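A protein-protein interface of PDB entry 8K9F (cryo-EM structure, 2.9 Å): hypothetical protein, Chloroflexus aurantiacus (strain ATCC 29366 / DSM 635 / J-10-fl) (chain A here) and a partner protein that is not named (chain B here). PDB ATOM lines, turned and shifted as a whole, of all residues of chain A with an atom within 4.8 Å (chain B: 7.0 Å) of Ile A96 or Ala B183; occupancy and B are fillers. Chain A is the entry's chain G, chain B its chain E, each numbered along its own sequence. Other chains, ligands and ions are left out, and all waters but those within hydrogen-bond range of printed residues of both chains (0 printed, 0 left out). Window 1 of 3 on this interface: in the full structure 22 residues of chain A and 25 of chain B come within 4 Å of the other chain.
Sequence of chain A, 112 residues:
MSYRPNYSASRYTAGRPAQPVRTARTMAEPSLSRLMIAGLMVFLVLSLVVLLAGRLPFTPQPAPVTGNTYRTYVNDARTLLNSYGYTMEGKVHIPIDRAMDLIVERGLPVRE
OG of Ser B187 sits at hydrogen-bond distance from O of Ile A94 (2.4 Å).
The backbone carbonyl oxygen of Leu A81 sits at hydrogen-bond distance from the backbone NH of Ile A96. OE1 of Gln B188 lies within hydrogen-bond range of OG of Ser B187 (3.1 Å).
Among the printed residues, merely in contact across the chains: Ile A94 with Leu B186, Met A100 with Leu B92, Ile A103 with Leu B186, Ile A103 with Leu B92, Leu A81 with Glu B109, Leu A81 with Tyr B180, Ile A96 with Ala B183, Ala A99 with Ser B187, Ile A96 with Ser B187, Met A100 with Lys B89, Ile A103 with Ala B183, Met A100 with Leu B93, Pro A95 with Ser B187, Ala A99 with Leu B186 and Leu A81 with Leu B184.
Ile A96 touches two residues of chain B. Ala B183 touches just these residues of chain A: Ile A96 and Ile A103. Of the printed residues of chain B, Ala A99 touches Leu B186 and Ser B187. Printed residues of chain A within 4 Å of Leu B92: Met A100 (3.3 Å) and Ile A103 (3.6 Å). The nearest residue of chain B that does not touch Ile A96 is Leu B184 (4.1 Å).
Of the 9 printed residues of chain A, 7 touch a printed residue of chain B. Hydrophobic or aromatic side chains of chain A within 4 Å of the printed part of chain B: Leu A81, Ile A94, Ile A96, Ala A99, Met A100 and Ile A103. Of the 18 printed residues of chain B, 9 touch a printed residue of chain A. Printed residues of chain B that touch a printed residue of chain A: Lys B89, Leu B92, Leu B93, Glu B109, Tyr B180, Ala B183, Leu B184, Leu B186 and Ser B187. Hydrophobic or aromatic side chains of chain B within 4 Å of the printed part of chain A: Leu B92, Tyr B180, Ala B183, Leu B184 and Leu B186.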
ATOM      1  N   LEU A  81       4.003 -32.138  15.570  1.00  0.00           N
ATOM      2  CA  LEU A  81       4.696 -32.038  16.847  1.00  0.00           C
ATOM      3  C   LEU A  81       6.156 -32.436  16.719  1.00  0.00           C
ATOM      4  O   LEU A  81       7.036 -31.712  17.189  1.00  0.00           O
ATOM      5  CB  LEU A  81       3.988 -32.885  17.904  1.00  0.00           C
ATOM      6  CG  LEU A  81       2.808 -32.223  18.623  1.00  0.00           C
ATOM      7  CD1 LEU A  81       2.527 -32.905  19.945  1.00  0.00           C
ATOM      8  CD2 LEU A  81       3.058 -30.738  18.850  1.00  0.00           C
ATOM      9  N   ILE A  94      10.611 -26.684  16.657  1.00  0.00           N
ATOM     10  CA  ILE A  94      11.421 -27.477  17.572  1.00  0.00           C
ATOM     11  C   ILE A  94      10.527 -28.599  18.089  1.00  0.00           C
ATOM     12  O   ILE A  94       9.438 -28.324  18.606  1.00  0.00           O
ATOM     13  CB  ILE A  94      12.002 -26.604  18.698  1.00  0.00           C
ATOM     14  CG1 ILE A  94      12.560 -25.297  18.122  1.00  0.00           C
ATOM     15  CG2 ILE A  94      13.063 -27.344  19.455  1.00  0.00           C
ATOM     16  CD1 ILE A  94      11.813 -24.047  18.509  1.00  0.00           C
ATOM     17  N   PRO A  95      10.911 -29.862  17.935  1.00  0.00           N
ATOM     18  CA  PRO A  95       9.989 -30.958  18.237  1.00  0.00           C
ATOM     19  C   PRO A  95       9.765 -31.156  19.728  1.00  0.00           C
ATOM     20  O   PRO A  95      10.629 -30.887  20.561  1.00  0.00           O
ATOM     21  CB  PRO A  95      10.680 -32.186  17.626  1.00  0.00           C
ATOM     22  CG  PRO A  95      11.709 -31.632  16.691  1.00  0.00           C
ATOM     23  CD  PRO A  95      12.156 -30.361  17.340  1.00  0.00           C
ATOM     24  N   ILE A  96       8.561 -31.630  20.043  1.00  0.00           N
ATOM     25  CA  ILE A  96       8.239 -32.080  21.391  1.00  0.00           C
ATOM     26  C   ILE A  96       9.111 -33.290  21.709  1.00  0.00           C
ATOM     27  O   ILE A  96       9.358 -34.127  20.829  1.00  0.00           O
ATOM     28  CB  ILE A  96       6.732 -32.376  21.483  1.00  0.00           C
ATOM     29  CG1 ILE A  96       5.946 -31.074  21.661  1.00  0.00           C
ATOM     30  CG2 ILE A  96       6.371 -33.353  22.590  1.00  0.00           C
ATOM     31  CD1 ILE A  96       6.384 -30.240  22.838  1.00  0.00           C
ATOM     32  N   ASP A  97       9.622 -33.343  22.949  1.00  0.00           N
ATOM     33  CA  ASP A  97      10.684 -34.177  23.557  1.00  0.00           C
ATOM     34  C   ASP A  97      12.061 -33.634  23.193  1.00  0.00           C
ATOM     35  O   ASP A  97      13.064 -34.160  23.687  1.00  0.00           O
ATOM     36  CB  ASP A  97      10.634 -35.679  23.214  1.00  0.00           C
ATOM     37  CG  ASP A  97       9.279 -36.295  23.479  1.00  0.00           C
ATOM     38  OD1 ASP A  97       8.698 -36.027  24.554  1.00  0.00           O
ATOM     39  OD2 ASP A  97       8.798 -37.053  22.608  1.00  0.00           O
ATOM     40  N   ARG A  98      12.143 -32.603  22.355  1.00  0.00           N
ATOM     41  CA  ARG A  98      13.370 -31.841  22.183  1.00  0.00           C
ATOM     42  C   ARG A  98      13.100 -30.431  22.685  1.00  0.00           C
ATOM     43  O   ARG A  98      13.901 -29.866  23.435  1.00  0.00           O
ATOM     44  CB  ARG A  98      13.827 -31.841  20.721  1.00  0.00           C
ATOM     45  CG  ARG A  98      15.120 -31.082  20.467  1.00  0.00           C
ATOM     46  CD  ARG A  98      15.560 -31.119  19.017  1.00  0.00           C
ATOM     47  NE  ARG A  98      16.804 -30.380  18.810  1.00  0.00           N
ATOM     48  CZ  ARG A  98      16.883 -29.076  18.579  1.00  0.00           C
ATOM     49  NH1 ARG A  98      15.803 -28.313  18.530  1.00  0.00           N
ATOM     50  NH2 ARG A  98      18.077 -28.520  18.395  1.00  0.00           N
ATOM     51  N   ALA A  99      11.955 -29.867  22.291  1.00  0.00           N
ATOM     52  CA  ALA A  99      11.513 -28.613  22.887  1.00  0.00           C
ATOM     53  C   ALA A  99      11.121 -28.806  24.339  1.00  0.00           C
ATOM     54  O   ALA A  99      11.209 -27.866  25.129  1.00  0.00           O
ATOM     55  CB  ALA A  99      10.341 -28.027  22.101  1.00  0.00           C
ATOM     56  N   MET A 100      10.675 -30.011  24.698  1.00  0.00           N
ATOM     57  CA  MET A 100      10.383 -30.342  26.088  1.00  0.00           C
ATOM     58  C   MET A 100      11.661 -30.338  26.920  1.00  0.00           C
ATOM     59  O   MET A 100      11.708 -29.766  28.017  1.00  0.00           O
ATOM     60  CB  MET A 100       9.702 -31.709  26.127  1.00  0.00           C
ATOM     61  CG  MET A 100       8.224 -31.681  25.746  1.00  0.00           C
ATOM     62  SD  MET A 100       7.326 -33.204  26.095  1.00  0.00           S
ATOM     63  CE  MET A 100       6.901 -33.013  27.801  1.00  0.00           C
ATOM     64  N   ILE A 103      12.730 -26.759  27.294  1.00  0.00           N
ATOM     65  CA  ILE A 103      11.955 -25.874  28.155  1.00  0.00           C
ATOM     66  C   ILE A 103      12.194 -26.246  29.618  1.00  0.00           C
ATOM     67  O   ILE A 103      12.125 -25.387  30.503  1.00  0.00           O
ATOM     68  CB  ILE A 103      10.454 -25.950  27.817  1.00  0.00           C
ATOM     69  CG1 ILE A 103       9.689 -24.831  28.528  1.00  0.00           C
ATOM     70  CG2 ILE A 103       9.891 -27.310  28.197  1.00  0.00           C
ATOM     71  CD1 ILE A 103      10.051 -23.444  28.047  1.00  0.00           C
ATOM     72  N   LYS B  89      11.251 -33.290  33.844  1.00  0.00           N
ATOM     73  CA  LYS B  89      10.795 -33.956  32.631  1.00  0.00           C
ATOM     74  C   LYS B  89       9.611 -34.875  32.905  1.00  0.00           C
ATOM     75  O   LYS B  89       8.728 -35.004  32.056  1.00  0.00           O
ATOM     76  CB  LYS B  89      11.942 -34.739  31.995  1.00  0.00           C
ATOM     77  CG  LYS B  89      11.653 -35.238  30.588  1.00  0.00           C
ATOM     78  CD  LYS B  89      11.167 -34.115  29.685  1.00  0.00           C
ATOM     79  CE  LYS B  89      10.743 -34.651  28.332  1.00  0.00           C
ATOM     80  NZ  LYS B  89      11.768 -35.566  27.764  1.00  0.00           N
ATOM     81  N   LEU B  92       6.741 -32.609  33.223  1.00  0.00           N
ATOM     82  CA  LEU B  92       6.427 -32.172  31.868  1.00  0.00           C
ATOM     83  C   LEU B  92       5.656 -33.239  31.097  1.00  0.00           C
ATOM     84  O   LEU B  92       4.717 -32.922  30.362  1.00  0.00           O
ATOM     85  CB  LEU B  92       7.728 -31.810  31.155  1.00  0.00           C
ATOM     86  CG  LEU B  92       7.840 -30.516  30.355  1.00  0.00           C
ATOM     87  CD1 LEU B  92       7.095 -29.407  31.013  1.00  0.00           C
ATOM     88  CD2 LEU B  92       9.297 -30.155  30.237  1.00  0.00           C
ATOM     89  N   LEU B  93       6.023 -34.511  31.263  1.00  0.00           N
ATOM     90  CA  LEU B  93       5.301 -35.592  30.597  1.00  0.00           C
ATOM     91  C   LEU B  93       3.937 -35.831  31.227  1.00  0.00           C
ATOM     92  O   LEU B  93       2.995 -36.226  30.531  1.00  0.00           O
ATOM     93  CB  LEU B  93       6.132 -36.874  30.626  1.00  0.00           C
ATOM     94  CG  LEU B  93       7.362 -36.894  29.719  1.00  0.00           C
ATOM     95  CD1 LEU B  93       8.407 -37.842  30.271  1.00  0.00           C
ATOM     96  CD2 LEU B  93       6.988 -37.279  28.299  1.00  0.00           C
ATOM     97  N   GLN B  96       1.945 -33.324  29.636  1.00  0.00           N
ATOM     98  CA  GLN B  96       1.639 -33.771  28.277  1.00  0.00           C
ATOM     99  C   GLN B  96       0.453 -34.720  28.256  1.00  0.00           C
ATOM    100  O   GLN B  96      -0.458 -34.575  27.433  1.00  0.00           O
ATOM    101  CB  GLN B  96       2.855 -34.459  27.663  1.00  0.00           C
ATOM    102  CG  GLN B  96       2.597 -35.028  26.280  1.00  0.00           C
ATOM    103  CD  GLN B  96       3.484 -36.195  25.959  1.00  0.00           C
ATOM    104  OE1 GLN B  96       3.955 -36.895  26.855  1.00  0.00           O
ATOM    105  NE2 GLN B  96       3.730 -36.413  24.674  1.00  0.00           N
ATOM    106  N   GLU B 109      -3.626 -31.393  19.177  1.00  0.00           N
ATOM    107  CA  GLU B 109      -2.384 -31.874  19.775  1.00  0.00           C
ATOM    108  C   GLU B 109      -1.246 -30.890  19.547  1.00  0.00           C
ATOM    109  O   GLU B 109      -0.361 -30.742  20.396  1.00  0.00           O
ATOM    110  CB  GLU B 109      -2.016 -33.247  19.211  1.00  0.00           C
ATOM    111  CG  GLU B 109      -3.130 -34.281  19.235  1.00  0.00           C
ATOM    112  CD  GLU B 109      -2.983 -35.258  20.387  1.00  0.00           C
ATOM    113  OE1 GLU B 109      -2.443 -36.361  20.164  1.00  0.00           O
ATOM    114  OE2 GLU B 109      -3.396 -34.925  21.516  1.00  0.00           O
ATOM    115  N   LEU B 138       2.096 -17.764  32.933  1.00  0.00           N
ATOM    116  CA  LEU B 138       1.685 -19.138  33.229  1.00  0.00           C
ATOM    117  C   LEU B 138       0.525 -19.181  34.213  1.00  0.00           C
ATOM    118  O   LEU B 138      -0.339 -20.071  34.133  1.00  0.00           O
ATOM    119  CB  LEU B 138       2.850 -19.955  33.795  1.00  0.00           C
ATOM    120  CG  LEU B 138       3.934 -20.536  32.881  1.00  0.00           C
ATOM    121  CD1 LEU B 138       3.315 -21.321  31.739  1.00  0.00           C
ATOM    122  CD2 LEU B 138       4.906 -19.498  32.375  1.00  0.00           C
ATOM    123  N   ILE B 177      -0.040 -28.935  33.164  1.00  0.00           N
ATOM    124  CA  ILE B 177      -0.648 -28.579  31.883  1.00  0.00           C
ATOM    125  C   ILE B 177      -0.160 -27.210  31.415  1.00  0.00           C
ATOM    126  O   ILE B 177       0.108 -27.013  30.226  1.00  0.00           O
ATOM    127  CB  ILE B 177      -2.186 -28.649  31.996  1.00  0.00           C
ATOM    128  CG1 ILE B 177      -2.644 -30.098  31.947  1.00  0.00           C
ATOM    129  CG2 ILE B 177      -2.883 -27.857  30.916  1.00  0.00           C
ATOM    130  CD1 ILE B 177      -4.143 -30.273  31.975  1.00  0.00           C
ATOM    131  N   ALA B 178      -0.006 -26.259  32.343  1.00  0.00           N
ATOM    132  CA  ALA B 178       0.560 -24.953  31.991  1.00  0.00           C
ATOM    133  C   ALA B 178       2.005 -25.072  31.508  1.00  0.00           C
ATOM    134  O   ALA B 178       2.420 -24.386  30.561  1.00  0.00           O
ATOM    135  CB  ALA B 178       0.480 -24.009  33.187  1.00  0.00           C
ATOM    136  N   ALA B 179       2.780 -25.949  32.146  1.00  0.00           N
ATOM    137  CA  ALA B 179       4.156 -26.187  31.722  1.00  0.00           C
ATOM    138  C   ALA B 179       4.218 -26.794  30.324  1.00  0.00           C
ATOM    139  O   ALA B 179       5.054 -26.398  29.502  1.00  0.00           O
ATOM    140  CB  ALA B 179       4.852 -27.093  32.730  1.00  0.00           C
ATOM    141  N   TYR B 180       3.333 -27.745  30.022  1.00  0.00           N
ATOM    142  CA  TYR B 180       3.334 -28.270  28.661  1.00  0.00           C
ATOM    143  C   TYR B 180       2.701 -27.303  27.663  1.00  0.00           C
ATOM    144  O   TYR B 180       3.015 -27.390  26.474  1.00  0.00           O
ATOM    145  CB  TYR B 180       2.700 -29.674  28.618  1.00  0.00           C
ATOM    146  CG  TYR B 180       2.531 -30.261  27.221  1.00  0.00           C
ATOM    147  CD1 TYR B 180       3.483 -31.122  26.698  1.00  0.00           C
ATOM    148  CD2 TYR B 180       1.360 -30.074  26.493  1.00  0.00           C
ATOM    149  CE1 TYR B 180       3.333 -31.673  25.440  1.00  0.00           C
ATOM    150  CE2 TYR B 180       1.205 -30.621  25.243  1.00  0.00           C
ATOM    151  CZ  TYR B 180       2.179 -31.435  24.728  1.00  0.00           C
ATOM    152  OH  TYR B 180       1.996 -31.990  23.486  1.00  0.00           O
ATOM    153  N   ILE B 181       1.866 -26.362  28.112  1.00  0.00           N
ATOM    154  CA  ILE B 181       1.461 -25.266  27.233  1.00  0.00           C
ATOM    155  C   ILE B 181       2.683 -24.475  26.813  1.00  0.00           C
ATOM    156  O   ILE B 181       2.871 -24.193  25.629  1.00  0.00           O
ATOM    157  CB  ILE B 181       0.438 -24.343  27.919  1.00  0.00           C
ATOM    158  CG1 ILE B 181      -0.957 -24.930  27.935  1.00  0.00           C
ATOM    159  CG2 ILE B 181       0.333 -23.014  27.195  1.00  0.00           C
ATOM    160  CD1 ILE B 181      -1.751 -24.334  29.055  1.00  0.00           C
ATOM    161  N   ARG B 182       3.551 -24.154  27.777  1.00  0.00           N
ATOM    162  CA  ARG B 182       4.769 -23.409  27.465  1.00  0.00           C
ATOM    163  C   ARG B 182       5.706 -24.221  26.575  1.00  0.00           C
ATOM    164  O   ARG B 182       6.353 -23.670  25.679  1.00  0.00           O
ATOM    165  CB  ARG B 182       5.475 -22.995  28.753  1.00  0.00           C
ATOM    166  CG  ARG B 182       6.302 -21.728  28.616  1.00  0.00           C
ATOM    167  CD  ARG B 182       5.508 -20.604  27.967  1.00  0.00           C
ATOM    168  NE  ARG B 182       4.700 -19.873  28.937  1.00  0.00           N
ATOM    169  CZ  ARG B 182       4.087 -18.724  28.688  1.00  0.00           C
ATOM    170  NH1 ARG B 182       4.185 -18.128  27.511  1.00  0.00           N
ATOM    171  NH2 ARG B 182       3.370 -18.149  29.647  1.00  0.00           N
ATOM    172  N   ALA B 183       5.758 -25.538  26.788  1.00  0.00           N
ATOM    173  CA  ALA B 183       6.505 -26.420  25.890  1.00  0.00           C
ATOM    174  C   ALA B 183       5.912 -26.426  24.487  1.00  0.00           C
ATOM    175  O   ALA B 183       6.642 -26.554  23.500  1.00  0.00           O
ATOM    176  CB  ALA B 183       6.529 -27.840  26.449  1.00  0.00           C
ATOM    177  N   LEU B 184       4.592 -26.293  24.380  1.00  0.00           N
ATOM    178  CA  LEU B 184       3.939 -26.291  23.079  1.00  0.00           C
ATOM    179  C   LEU B 184       4.162 -24.979  22.342  1.00  0.00           C
ATOM    180  O   LEU B 184       4.380 -24.977  21.125  1.00  0.00           O
ATOM    181  CB  LEU B 184       2.448 -26.555  23.258  1.00  0.00           C
ATOM    182  CG  LEU B 184       1.827 -27.524  22.266  1.00  0.00           C
ATOM    183  CD1 LEU B 184       2.564 -28.849  22.311  1.00  0.00           C
ATOM    184  CD2 LEU B 184       0.373 -27.709  22.602  1.00  0.00           C
ATOM    185  N   GLN B 185       4.076 -23.855  23.060  1.00  0.00           N
ATOM    186  CA  GLN B 185       4.367 -22.550  22.469  1.00  0.00           C
ATOM    187  C   GLN B 185       5.826 -22.442  22.061  1.00  0.00           C
ATOM    188  O   GLN B 185       6.134 -21.902  20.992  1.00  0.00           O
ATOM    189  CB  GLN B 185       4.012 -21.418  23.431  1.00  0.00           C
ATOM    190  CG  GLN B 185       2.635 -21.487  24.047  1.00  0.00           C
ATOM    191  CD  GLN B 185       2.081 -20.130  24.381  1.00  0.00           C
ATOM    192  OE1 GLN B 185       1.449 -19.488  23.556  1.00  0.00           O
ATOM    193  NE2 GLN B 185       2.319 -19.682  25.606  1.00  0.00           N
ATOM    194  N   LEU B 186       6.740 -22.945  22.894  1.00  0.00           N
ATOM    195  CA  LEU B 186       8.150 -22.965  22.536  1.00  0.00           C
ATOM    196  C   LEU B 186       8.427 -23.957  21.417  1.00  0.00           C
ATOM    197  O   LEU B 186       9.380 -23.763  20.661  1.00  0.00           O
ATOM    198  CB  LEU B 186       9.006 -23.302  23.758  1.00  0.00           C
ATOM    199  CG  LEU B 186      10.513 -23.429  23.516  1.00  0.00           C
ATOM    200  CD1 LEU B 186      11.094 -22.104  23.045  1.00  0.00           C
ATOM    201  CD2 LEU B 186      11.221 -23.915  24.771  1.00  0.00           C
ATOM    202  N   SER B 187       7.605 -24.998  21.285  1.00  0.00           N
ATOM    203  CA  SER B 187       7.808 -25.977  20.225  1.00  0.00           C
ATOM    204  C   SER B 187       7.414 -25.420  18.865  1.00  0.00           C
ATOM    205  O   SER B 187       7.950 -25.844  17.836  1.00  0.00           O
ATOM    206  CB  SER B 187       7.010 -27.241  20.527  1.00  0.00           C
ATOM    207  OG  SER B 187       7.161 -28.184  19.484  1.00  0.00           O
ATOM    208  N   GLN B 188       6.475 -24.482  18.835  1.00  0.00           N
ATOM    209  CA  GLN B 188       5.926 -23.976  17.587  1.00  0.00           C
ATOM    210  C   GLN B 188       6.393 -22.568  17.252  1.00  0.00           C
ATOM    211  O   GLN B 188       6.001 -22.032  16.212  1.00  0.00           O
ATOM    212  CB  GLN B 188       4.396 -24.022  17.638  1.00  0.00           C
ATOM    213  CG  GLN B 188       3.805 -25.424  17.788  1.00  0.00           C
ATOM    214  CD  GLN B 188       4.461 -26.453  16.885  1.00  0.00           C
ATOM    215  OE1 GLN B 188       4.963 -27.474  17.354  1.00  0.00           O
ATOM    216  NE2 GLN B 188       4.425 -26.206  15.577  1.00  0.00           N
